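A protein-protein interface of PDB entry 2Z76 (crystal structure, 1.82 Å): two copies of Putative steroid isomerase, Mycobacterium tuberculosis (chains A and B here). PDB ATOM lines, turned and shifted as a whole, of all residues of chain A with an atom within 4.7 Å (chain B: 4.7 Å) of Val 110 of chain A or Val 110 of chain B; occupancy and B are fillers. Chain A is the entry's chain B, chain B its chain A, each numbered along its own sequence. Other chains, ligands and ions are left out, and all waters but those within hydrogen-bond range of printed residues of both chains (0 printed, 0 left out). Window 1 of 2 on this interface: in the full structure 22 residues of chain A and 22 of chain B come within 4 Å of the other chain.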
ATOM      1  N   PHE A  81      -9.745 -15.496 -10.976  1.00  0.00           N
ATOM      2  CA  PHE A  81      -9.255 -16.152  -9.770  1.00  0.00           C
ATOM      3  C   PHE A  81      -8.990 -17.639 -10.015  1.00  0.00           C
ATOM      4  O   PHE A  81      -9.911 -18.457  -9.934  1.00  0.00           O
ATOM      5  CB  PHE A  81     -10.276 -15.980  -8.637  1.00  0.00           C
ATOM      6  CG  PHE A  81     -10.464 -14.558  -8.215  1.00  0.00           C
ATOM      7  CD1 PHE A  81      -9.665 -14.018  -7.195  1.00  0.00           C
ATOM      8  CD2 PHE A  81     -11.410 -13.738  -8.851  1.00  0.00           C
ATOM      9  CE1 PHE A  81      -9.837 -12.703  -6.795  1.00  0.00           C
ATOM     10  CE2 PHE A  81     -11.593 -12.409  -8.445  1.00  0.00           C
ATOM     11  CZ  PHE A  81     -10.807 -11.896  -7.419  1.00  0.00           C
ATOM     12  N   ALA A  90     -12.566 -19.244 -11.325  1.00  0.00           N
ATOM     13  CA  ALA A  90     -13.639 -18.265 -11.079  1.00  0.00           C
ATOM     14  C   ALA A  90     -13.290 -16.938 -11.732  1.00  0.00           C
ATOM     15  O   ALA A  90     -12.111 -16.588 -11.836  1.00  0.00           O
ATOM     16  CB  ALA A  90     -13.897 -18.069  -9.545  1.00  0.00           C
ATOM     17  N   HIS A  91     -14.307 -16.179 -12.152  1.00  0.00           N
ATOM     18  CA  HIS A  91     -14.101 -14.867 -12.752  1.00  0.00           C
ATOM     19  C   HIS A  91     -15.130 -13.853 -12.255  1.00  0.00           C
ATOM     20  O   HIS A  91     -16.250 -14.219 -11.848  1.00  0.00           O
ATOM     21  CB  HIS A  91     -14.220 -14.925 -14.294  1.00  0.00           C
ATOM     22  CG  HIS A  91     -13.367 -15.951 -14.965  1.00  0.00           C
ATOM     23  ND1 HIS A  91     -12.092 -15.678 -15.411  1.00  0.00           N
ATOM     24  CD2 HIS A  91     -13.633 -17.223 -15.341  1.00  0.00           C
ATOM     25  CE1 HIS A  91     -11.597 -16.752 -15.992  1.00  0.00           C
ATOM     26  NE2 HIS A  91     -12.515 -17.699 -15.973  1.00  0.00           N
ATOM     27  N   ILE A  92     -14.756 -12.582 -12.259  1.00  0.00           N
ATOM     28  CA  ILE A  92     -15.741 -11.509 -12.134  1.00  0.00           C
ATOM     29  C   ILE A  92     -16.060 -11.062 -13.579  1.00  0.00           C
ATOM     30  O   ILE A  92     -15.174 -10.568 -14.286  1.00  0.00           O
ATOM     31  CB  ILE A  92     -15.255 -10.326 -11.264  1.00  0.00           C
ATOM     32  CG1 ILE A  92     -15.019 -10.782  -9.807  1.00  0.00           C
ATOM     33  CG2 ILE A  92     -16.285  -9.182 -11.273  1.00  0.00           C
ATOM     34  CD1 ILE A  92     -14.467  -9.687  -8.902  1.00  0.00           C
ATOM     35  N   GLY A 109     -21.338 -10.247 -11.937  1.00  0.00           N
ATOM     36  CA  GLY A 109     -21.380 -11.334 -10.947  1.00  0.00           C
ATOM     37  C   GLY A 109     -20.115 -12.173 -10.968  1.00  0.00           C
ATOM     38  O   GLY A 109     -19.177 -11.896 -11.723  1.00  0.00           O
ATOM     39  N   VAL A 110     -20.096 -13.198 -10.134  1.00  0.00           N
ATOM     40  CA  VAL A 110     -18.984 -14.157 -10.112  1.00  0.00           C
ATOM     41  C   VAL A 110     -19.429 -15.359 -10.942  1.00  0.00           C
ATOM     42  O   VAL A 110     -20.564 -15.826 -10.809  1.00  0.00           O
ATOM     43  CB  VAL A 110     -18.687 -14.626  -8.660  1.00  0.00           C
ATOM     44  CG1 VAL A 110     -17.781 -15.849  -8.664  1.00  0.00           C
ATOM     45  CG2 VAL A 110     -18.054 -13.470  -7.833  1.00  0.00           C
ATOM     46  N   PHE A 111     -18.540 -15.857 -11.786  1.00  0.00           N
ATOM     47  CA  PHE A 111     -18.839 -17.040 -12.578  1.00  0.00           C
ATOM     48  C   PHE A 111     -17.794 -18.128 -12.375  1.00  0.00           C
ATOM     49  O   PHE A 111     -16.600 -17.867 -12.496  1.00  0.00           O
ATOM     50  CB  PHE A 111     -18.965 -16.673 -14.053  1.00  0.00           C
ATOM     51  CG  PHE A 111     -20.072 -15.677 -14.318  1.00  0.00           C
ATOM     52  CD1 PHE A 111     -21.289 -16.109 -14.839  1.00  0.00           C
ATOM     53  CD2 PHE A 111     -19.901 -14.329 -14.007  1.00  0.00           C
ATOM     54  CE1 PHE A 111     -22.334 -15.179 -15.062  1.00  0.00           C
ATOM     55  CE2 PHE A 111     -20.931 -13.407 -14.200  1.00  0.00           C
ATOM     56  CZ  PHE A 111     -22.143 -13.850 -14.743  1.00  0.00           C
ATOM     57  N   THR A 112     -18.254 -19.328 -12.054  1.00  0.00           N
ATOM     58  CA  THR A 112     -17.346 -20.437 -11.823  1.00  0.00           C
ATOM     59  C   THR A 112     -17.401 -21.411 -12.996  1.00  0.00           C
ATOM     60  O   THR A 112     -18.460 -21.597 -13.599  1.00  0.00           O
ATOM     61  CB  THR A 112     -17.550 -21.122 -10.430  1.00  0.00           C
ATOM     62  OG1 THR A 112     -18.837 -21.764 -10.343  1.00  0.00           O
ATOM     63  CG2 THR A 112     -17.389 -20.100  -9.308  1.00  0.00           C
ATOM     64  N   ARG A 125     -21.428 -21.760 -13.566  1.00  0.00           N
ATOM     65  CA  ARG A 125     -22.360 -21.365 -12.490  1.00  0.00           C
ATOM     66  C   ARG A 125     -22.182 -19.878 -12.195  1.00  0.00           C
ATOM     67  O   ARG A 125     -21.051 -19.399 -11.982  1.00  0.00           O
ATOM     68  CB  ARG A 125     -22.107 -22.179 -11.217  1.00  0.00           C
ATOM     69  CG  ARG A 125     -21.974 -23.690 -11.451  1.00  0.00           C
ATOM     70  CD  ARG A 125     -22.000 -24.439 -10.133  1.00  0.00           C
ATOM     71  NE  ARG A 125     -23.367 -24.614  -9.637  1.00  0.00           N
ATOM     72  CZ  ARG A 125     -23.748 -24.331  -8.396  1.00  0.00           C
ATOM     73  NH1 ARG A 125     -22.852 -23.915  -7.516  1.00  0.00           N
ATOM     74  NH2 ARG A 125     -24.996 -24.536  -8.007  1.00  0.00           N
ATOM     75  N   GLY A 126     -23.293 -19.149 -12.205  1.00  0.00           N
ATOM     76  CA  GLY A 126     -23.247 -17.706 -12.090  1.00  0.00           C
ATOM     77  C   GLY A 126     -23.930 -17.194 -10.836  1.00  0.00           C
ATOM     78  O   GLY A 126     -25.072 -17.573 -10.524  1.00  0.00           O
ATOM     79  N   TYR A 127     -23.214 -16.347 -10.091  1.00  0.00           N
ATOM     80  CA  TYR A 127     -23.741 -15.750  -8.872  1.00  0.00           C
ATOM     81  C   TYR A 127     -24.221 -14.356  -9.224  1.00  0.00           C
ATOM     82  O   TYR A 127     -23.458 -13.377  -9.211  1.00  0.00           O
ATOM     83  CB  TYR A 127     -22.675 -15.700  -7.740  1.00  0.00           C
ATOM     84  CG  TYR A 127     -22.238 -17.080  -7.310  1.00  0.00           C
ATOM     85  CD1 TYR A 127     -22.770 -17.676  -6.154  1.00  0.00           C
ATOM     86  CD2 TYR A 127     -21.295 -17.798  -8.061  1.00  0.00           C
ATOM     87  CE1 TYR A 127     -22.400 -18.939  -5.770  1.00  0.00           C
ATOM     88  CE2 TYR A 127     -20.895 -19.048  -7.673  1.00  0.00           C
ATOM     89  CZ  TYR A 127     -21.434 -19.618  -6.526  1.00  0.00           C
ATOM     90  OH  TYR A 127     -21.087 -20.889  -6.121  1.00  0.00           O
ATOM     91  N   PHE B  81     -21.600 -11.472  -3.629  1.00  0.00           N
ATOM     92  CA  PHE B  81     -22.304 -11.722  -4.864  1.00  0.00           C
ATOM     93  C   PHE B  81     -23.388 -12.771  -4.602  1.00  0.00           C
ATOM     94  O   PHE B  81     -23.099 -13.987  -4.651  1.00  0.00           O
ATOM     95  CB  PHE B  81     -21.317 -12.233  -5.916  1.00  0.00           C
ATOM     96  CG  PHE B  81     -20.349 -11.185  -6.433  1.00  0.00           C
ATOM     97  CD1 PHE B  81     -20.687 -10.410  -7.538  1.00  0.00           C
ATOM     98  CD2 PHE B  81     -19.087 -11.002  -5.849  1.00  0.00           C
ATOM     99  CE1 PHE B  81     -19.807  -9.457  -8.066  1.00  0.00           C
ATOM    100  CE2 PHE B  81     -18.204 -10.034  -6.376  1.00  0.00           C
ATOM    101  CZ  PHE B  81     -18.566  -9.276  -7.478  1.00  0.00           C
ATOM    102  N   ALA B  90     -21.437 -16.092  -3.252  1.00  0.00           N
ATOM    103  CA  ALA B  90     -19.991 -15.984  -3.435  1.00  0.00           C
ATOM    104  C   ALA B  90     -19.511 -14.666  -2.842  1.00  0.00           C
ATOM    105  O   ALA B  90     -20.269 -13.691  -2.760  1.00  0.00           O
ATOM    106  CB  ALA B  90     -19.627 -16.077  -4.917  1.00  0.00           C
ATOM    107  N   HIS B  91     -18.253 -14.639  -2.411  1.00  0.00           N
ATOM    108  CA  HIS B  91     -17.655 -13.425  -1.873  1.00  0.00           C
ATOM    109  C   HIS B  91     -16.210 -13.316  -2.367  1.00  0.00           C
ATOM    110  O   HIS B  91     -15.554 -14.343  -2.581  1.00  0.00           O
ATOM    111  CB  HIS B  91     -17.571 -13.471  -0.350  1.00  0.00           C
ATOM    112  CG  HIS B  91     -18.846 -13.780   0.354  1.00  0.00           C
ATOM    113  ND1 HIS B  91     -19.711 -12.801   0.753  1.00  0.00           N
ATOM    114  CD2 HIS B  91     -19.357 -14.950   0.819  1.00  0.00           C
ATOM    115  CE1 HIS B  91     -20.709 -13.345   1.430  1.00  0.00           C
ATOM    116  NE2 HIS B  91     -20.509 -14.653   1.480  1.00  0.00           N
ATOM    117  N   ILE B  92     -15.725 -12.088  -2.518  1.00  0.00           N
ATOM    118  CA  ILE B  92     -14.284 -11.816  -2.568  1.00  0.00           C
ATOM    119  C   ILE B  92     -13.838 -11.535  -1.141  1.00  0.00           C
ATOM    120  O   ILE B  92     -14.297 -10.585  -0.507  1.00  0.00           O
ATOM    121  CB  ILE B  92     -13.933 -10.594  -3.456  1.00  0.00           C
ATOM    122  CG1 ILE B  92     -14.626 -10.689  -4.816  1.00  0.00           C
ATOM    123  CG2 ILE B  92     -12.378 -10.422  -3.569  1.00  0.00           C
ATOM    124  CD1 ILE B  92     -14.375 -11.944  -5.567  1.00  0.00           C
ATOM    125  N   GLY B 109      -9.228 -14.042  -2.603  1.00  0.00           N
ATOM    126  CA  GLY B 109      -9.786 -14.934  -3.617  1.00  0.00           C
ATOM    127  C   GLY B 109     -11.292 -14.945  -3.554  1.00  0.00           C
ATOM    128  O   GLY B 109     -11.881 -14.223  -2.768  1.00  0.00           O
ATOM    129  N   VAL B 110     -11.887 -15.751  -4.423  1.00  0.00           N
ATOM    130  CA  VAL B 110     -13.320 -15.949  -4.450  1.00  0.00           C
ATOM    131  C   VAL B 110     -13.618 -17.145  -3.579  1.00  0.00           C
ATOM    132  O   VAL B 110     -12.932 -18.168  -3.697  1.00  0.00           O
ATOM    133  CB  VAL B 110     -13.835 -16.203  -5.904  1.00  0.00           C
ATOM    134  CG1 VAL B 110     -15.259 -16.716  -5.886  1.00  0.00           C
ATOM    135  CG2 VAL B 110     -13.706 -14.938  -6.748  1.00  0.00           C
ATOM    136  N   PHE B 111     -14.606 -17.007  -2.695  1.00  0.00           N
ATOM    137  CA  PHE B 111     -15.045 -18.128  -1.858  1.00  0.00           C
ATOM    138  C   PHE B 111     -16.537 -18.307  -2.048  1.00  0.00           C
ATOM    139  O   PHE B 111     -17.328 -17.332  -1.883  1.00  0.00           O
ATOM    140  CB  PHE B 111     -14.748 -17.871  -0.365  1.00  0.00           C
ATOM    141  CG  PHE B 111     -13.288 -17.833  -0.059  1.00  0.00           C
ATOM    142  CD1 PHE B 111     -12.667 -18.906   0.520  1.00  0.00           C
ATOM    143  CD2 PHE B 111     -12.523 -16.746  -0.448  1.00  0.00           C
ATOM    144  CE1 PHE B 111     -11.269 -18.849   0.766  1.00  0.00           C
ATOM    145  CE2 PHE B 111     -11.159 -16.695  -0.208  1.00  0.00           C
ATOM    146  CZ  PHE B 111     -10.549 -17.742   0.385  1.00  0.00           C
ATOM    147  N   THR B 112     -16.922 -19.535  -2.361  1.00  0.00           N
ATOM    148  CA  THR B 112     -18.328 -19.853  -2.567  1.00  0.00           C
ATOM    149  C   THR B 112     -18.845 -20.693  -1.394  1.00  0.00           C
ATOM    150  O   THR B 112     -18.120 -21.518  -0.821  1.00  0.00           O
ATOM    151  CB  THR B 112     -18.555 -20.566  -3.944  1.00  0.00           C
ATOM    152  OG1 THR B 112     -17.928 -21.858  -3.950  1.00  0.00           O
ATOM    153  CG2 THR B 112     -18.021 -19.697  -5.091  1.00  0.00           C
ATOM    154  N   ARG B 125     -15.832 -23.215  -0.667  1.00  0.00           N
ATOM    155  CA  ARG B 125     -14.845 -23.515  -1.725  1.00  0.00           C
ATOM    156  C   ARG B 125     -14.056 -22.277  -2.073  1.00  0.00           C
ATOM    157  O   ARG B 125     -14.647 -21.223  -2.356  1.00  0.00           O
ATOM    158  CB  ARG B 125     -15.504 -24.086  -2.999  1.00  0.00           C
ATOM    159  CG  ARG B 125     -16.544 -25.175  -2.765  1.00  0.00           C
ATOM    160  CD  ARG B 125     -17.035 -25.766  -4.091  1.00  0.00           C
ATOM    161  NE  ARG B 125     -16.045 -26.741  -4.576  1.00  0.00           N
ATOM    162  CZ  ARG B 125     -15.647 -26.887  -5.846  1.00  0.00           C
ATOM    163  NH1 ARG B 125     -16.115 -26.093  -6.809  1.00  0.00           N
ATOM    164  NH2 ARG B 125     -14.755 -27.840  -6.143  1.00  0.00           N
ATOM    165  N   GLY B 126     -12.733 -22.385  -2.042  1.00  0.00           N
ATOM    166  CA  GLY B 126     -11.896 -21.219  -2.287  1.00  0.00           C
ATOM    167  C   GLY B 126     -11.115 -21.297  -3.585  1.00  0.00           C
ATOM    168  O   GLY B 126     -10.501 -22.332  -3.902  1.00  0.00           O
ATOM    169  N   TYR B 127     -11.155 -20.190  -4.324  1.00  0.00           N
ATOM    170  CA  TYR B 127     -10.373 -20.010  -5.534  1.00  0.00           C
ATOM    171  C   TYR B 127      -9.118 -19.206  -5.248  1.00  0.00           C
ATOM    172  O   TYR B 127      -9.086 -17.988  -5.310  1.00  0.00           O
ATOM    173  CB  TYR B 127     -11.214 -19.382  -6.659  1.00  0.00           C
ATOM    174  CG  TYR B 127     -12.368 -20.251  -7.098  1.00  0.00           C
ATOM    175  CD1 TYR B 127     -12.266 -21.063  -8.247  1.00  0.00           C
ATOM    176  CD2 TYR B 127     -13.570 -20.270  -6.371  1.00  0.00           C
ATOM    177  CE1 TYR B 127     -13.329 -21.895  -8.635  1.00  0.00           C
ATOM    178  CE2 TYR B 127     -14.633 -21.080  -6.762  1.00  0.00           C
ATOM    179  CZ  TYR B 127     -14.512 -21.881  -7.903  1.00  0.00           C
ATOM    180  OH  TYR B 127     -15.557 -22.678  -8.293  1.00  0.00           O
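Phe 81 of chain A touches Gly 109 of chain B.
Phe 81 of chain A touches Val 110 of chain B (CD2 to CG2, 3.3 Å).
Ala 90 of chain A touches Tyr 127 of chain B (N to CD1, 3.6 Å).
CD1 of Phe 81 of chain B touches CA of Gly 109 of chain A (3.6 Å).
Val 110 of chain A touches Phe 81 of chain B (CG2 to CD2, 3.3 Å).
CG1 of Val 110 of chain A touches CG1 of Val 110 of chain B, at 3.9 Å.
Thr 112 of chain A touches Tyr 127 of chain B.
Tyr 127 of chain A touches Phe 81 of chain B (CB to O, 3.6 Å).
Tyr 127 of chain A touches Ala 90 of chain B.
Thr 112 of chain B touches Tyr 127 of chain A.
Phe 81 of chain A touches Tyr 127 of chain B, and with the chains exchanged Tyr 127 of chain A touches Phe 81 of chain B.
Ala 90 of chain A touches Tyr 127 of chain B, and with the chains exchanged Tyr 127 of chain A touches Ala 90 of chain B.
Val 110 of chain B touches its own counterpart, Val 110 of chain A.
Thr 112 of chain A touches Tyr 127 of chain B, and with the chains exchanged Tyr 127 of chain A touches Thr 112 of chain B.
11 positions are printed for both chains.
Hydrophobic or aromatic side chains of chain B that line the printed part of chain A: Phe 81, Ala 90, Val 110 and Tyr 127.
Among the printed residues, 11 pairs touch across the chains.
Among the printed residues, no Asp or Glu carboxylate lies within 4 Å of a Lys or Arg side-chain nitrogen of the other chain.
Val 110 of chain A touches just these residues of chain B: Phe 81 and Val 110.
Of the printed residues of chain A, Phe 81 of chain B touches Gly 109 (3.6 Å), Val 110 (3.3 Å) and Tyr 127 (3.6 Å).
Printed residues of chain A within 4 Å of Ala 90 of chain B: Tyr 127 (3.6 Å).
Val 110 of chain B touches just these residues of chain A: Phe 81 and Val 110.
The nearest residue of chain B that does not touch Val 110 of chain A is Ala 90 of chain B (4.1 Å).
The nearest residue of chain A that does not touch Val 110 of chain B is Ala 90 of chain A (4.1 Å).
The backbone NH (N) of Phe 81 of chain B sits at hydrogen-bond distance from the backbone carbonyl oxygen (O) of Ala 90 of chain B (2.7 Å).
O of Val 110 of chain B is in hydrogen-bond range of N of Tyr 127 of chain B (2.8 Å).
O of Arg 125 of chain B sits at hydrogen-bond distance from N of Thr 112 of chain B, at 2.8 Å.
N of Phe 81 of chain A is in hydrogen-bond range of O of Ala 90 of chain A (2.7 Å).
The backbone carbonyl oxygen (O) of Val 110 of chain A sits at hydrogen-bond distance from the backbone NH (N) of Tyr 127 of chain A (2.8 Å).
The backbone NH of Thr 112 of chain A lies within hydrogen-bond range of the backbone carbonyl oxygen of Arg 125 of chain A (2.8 Å).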
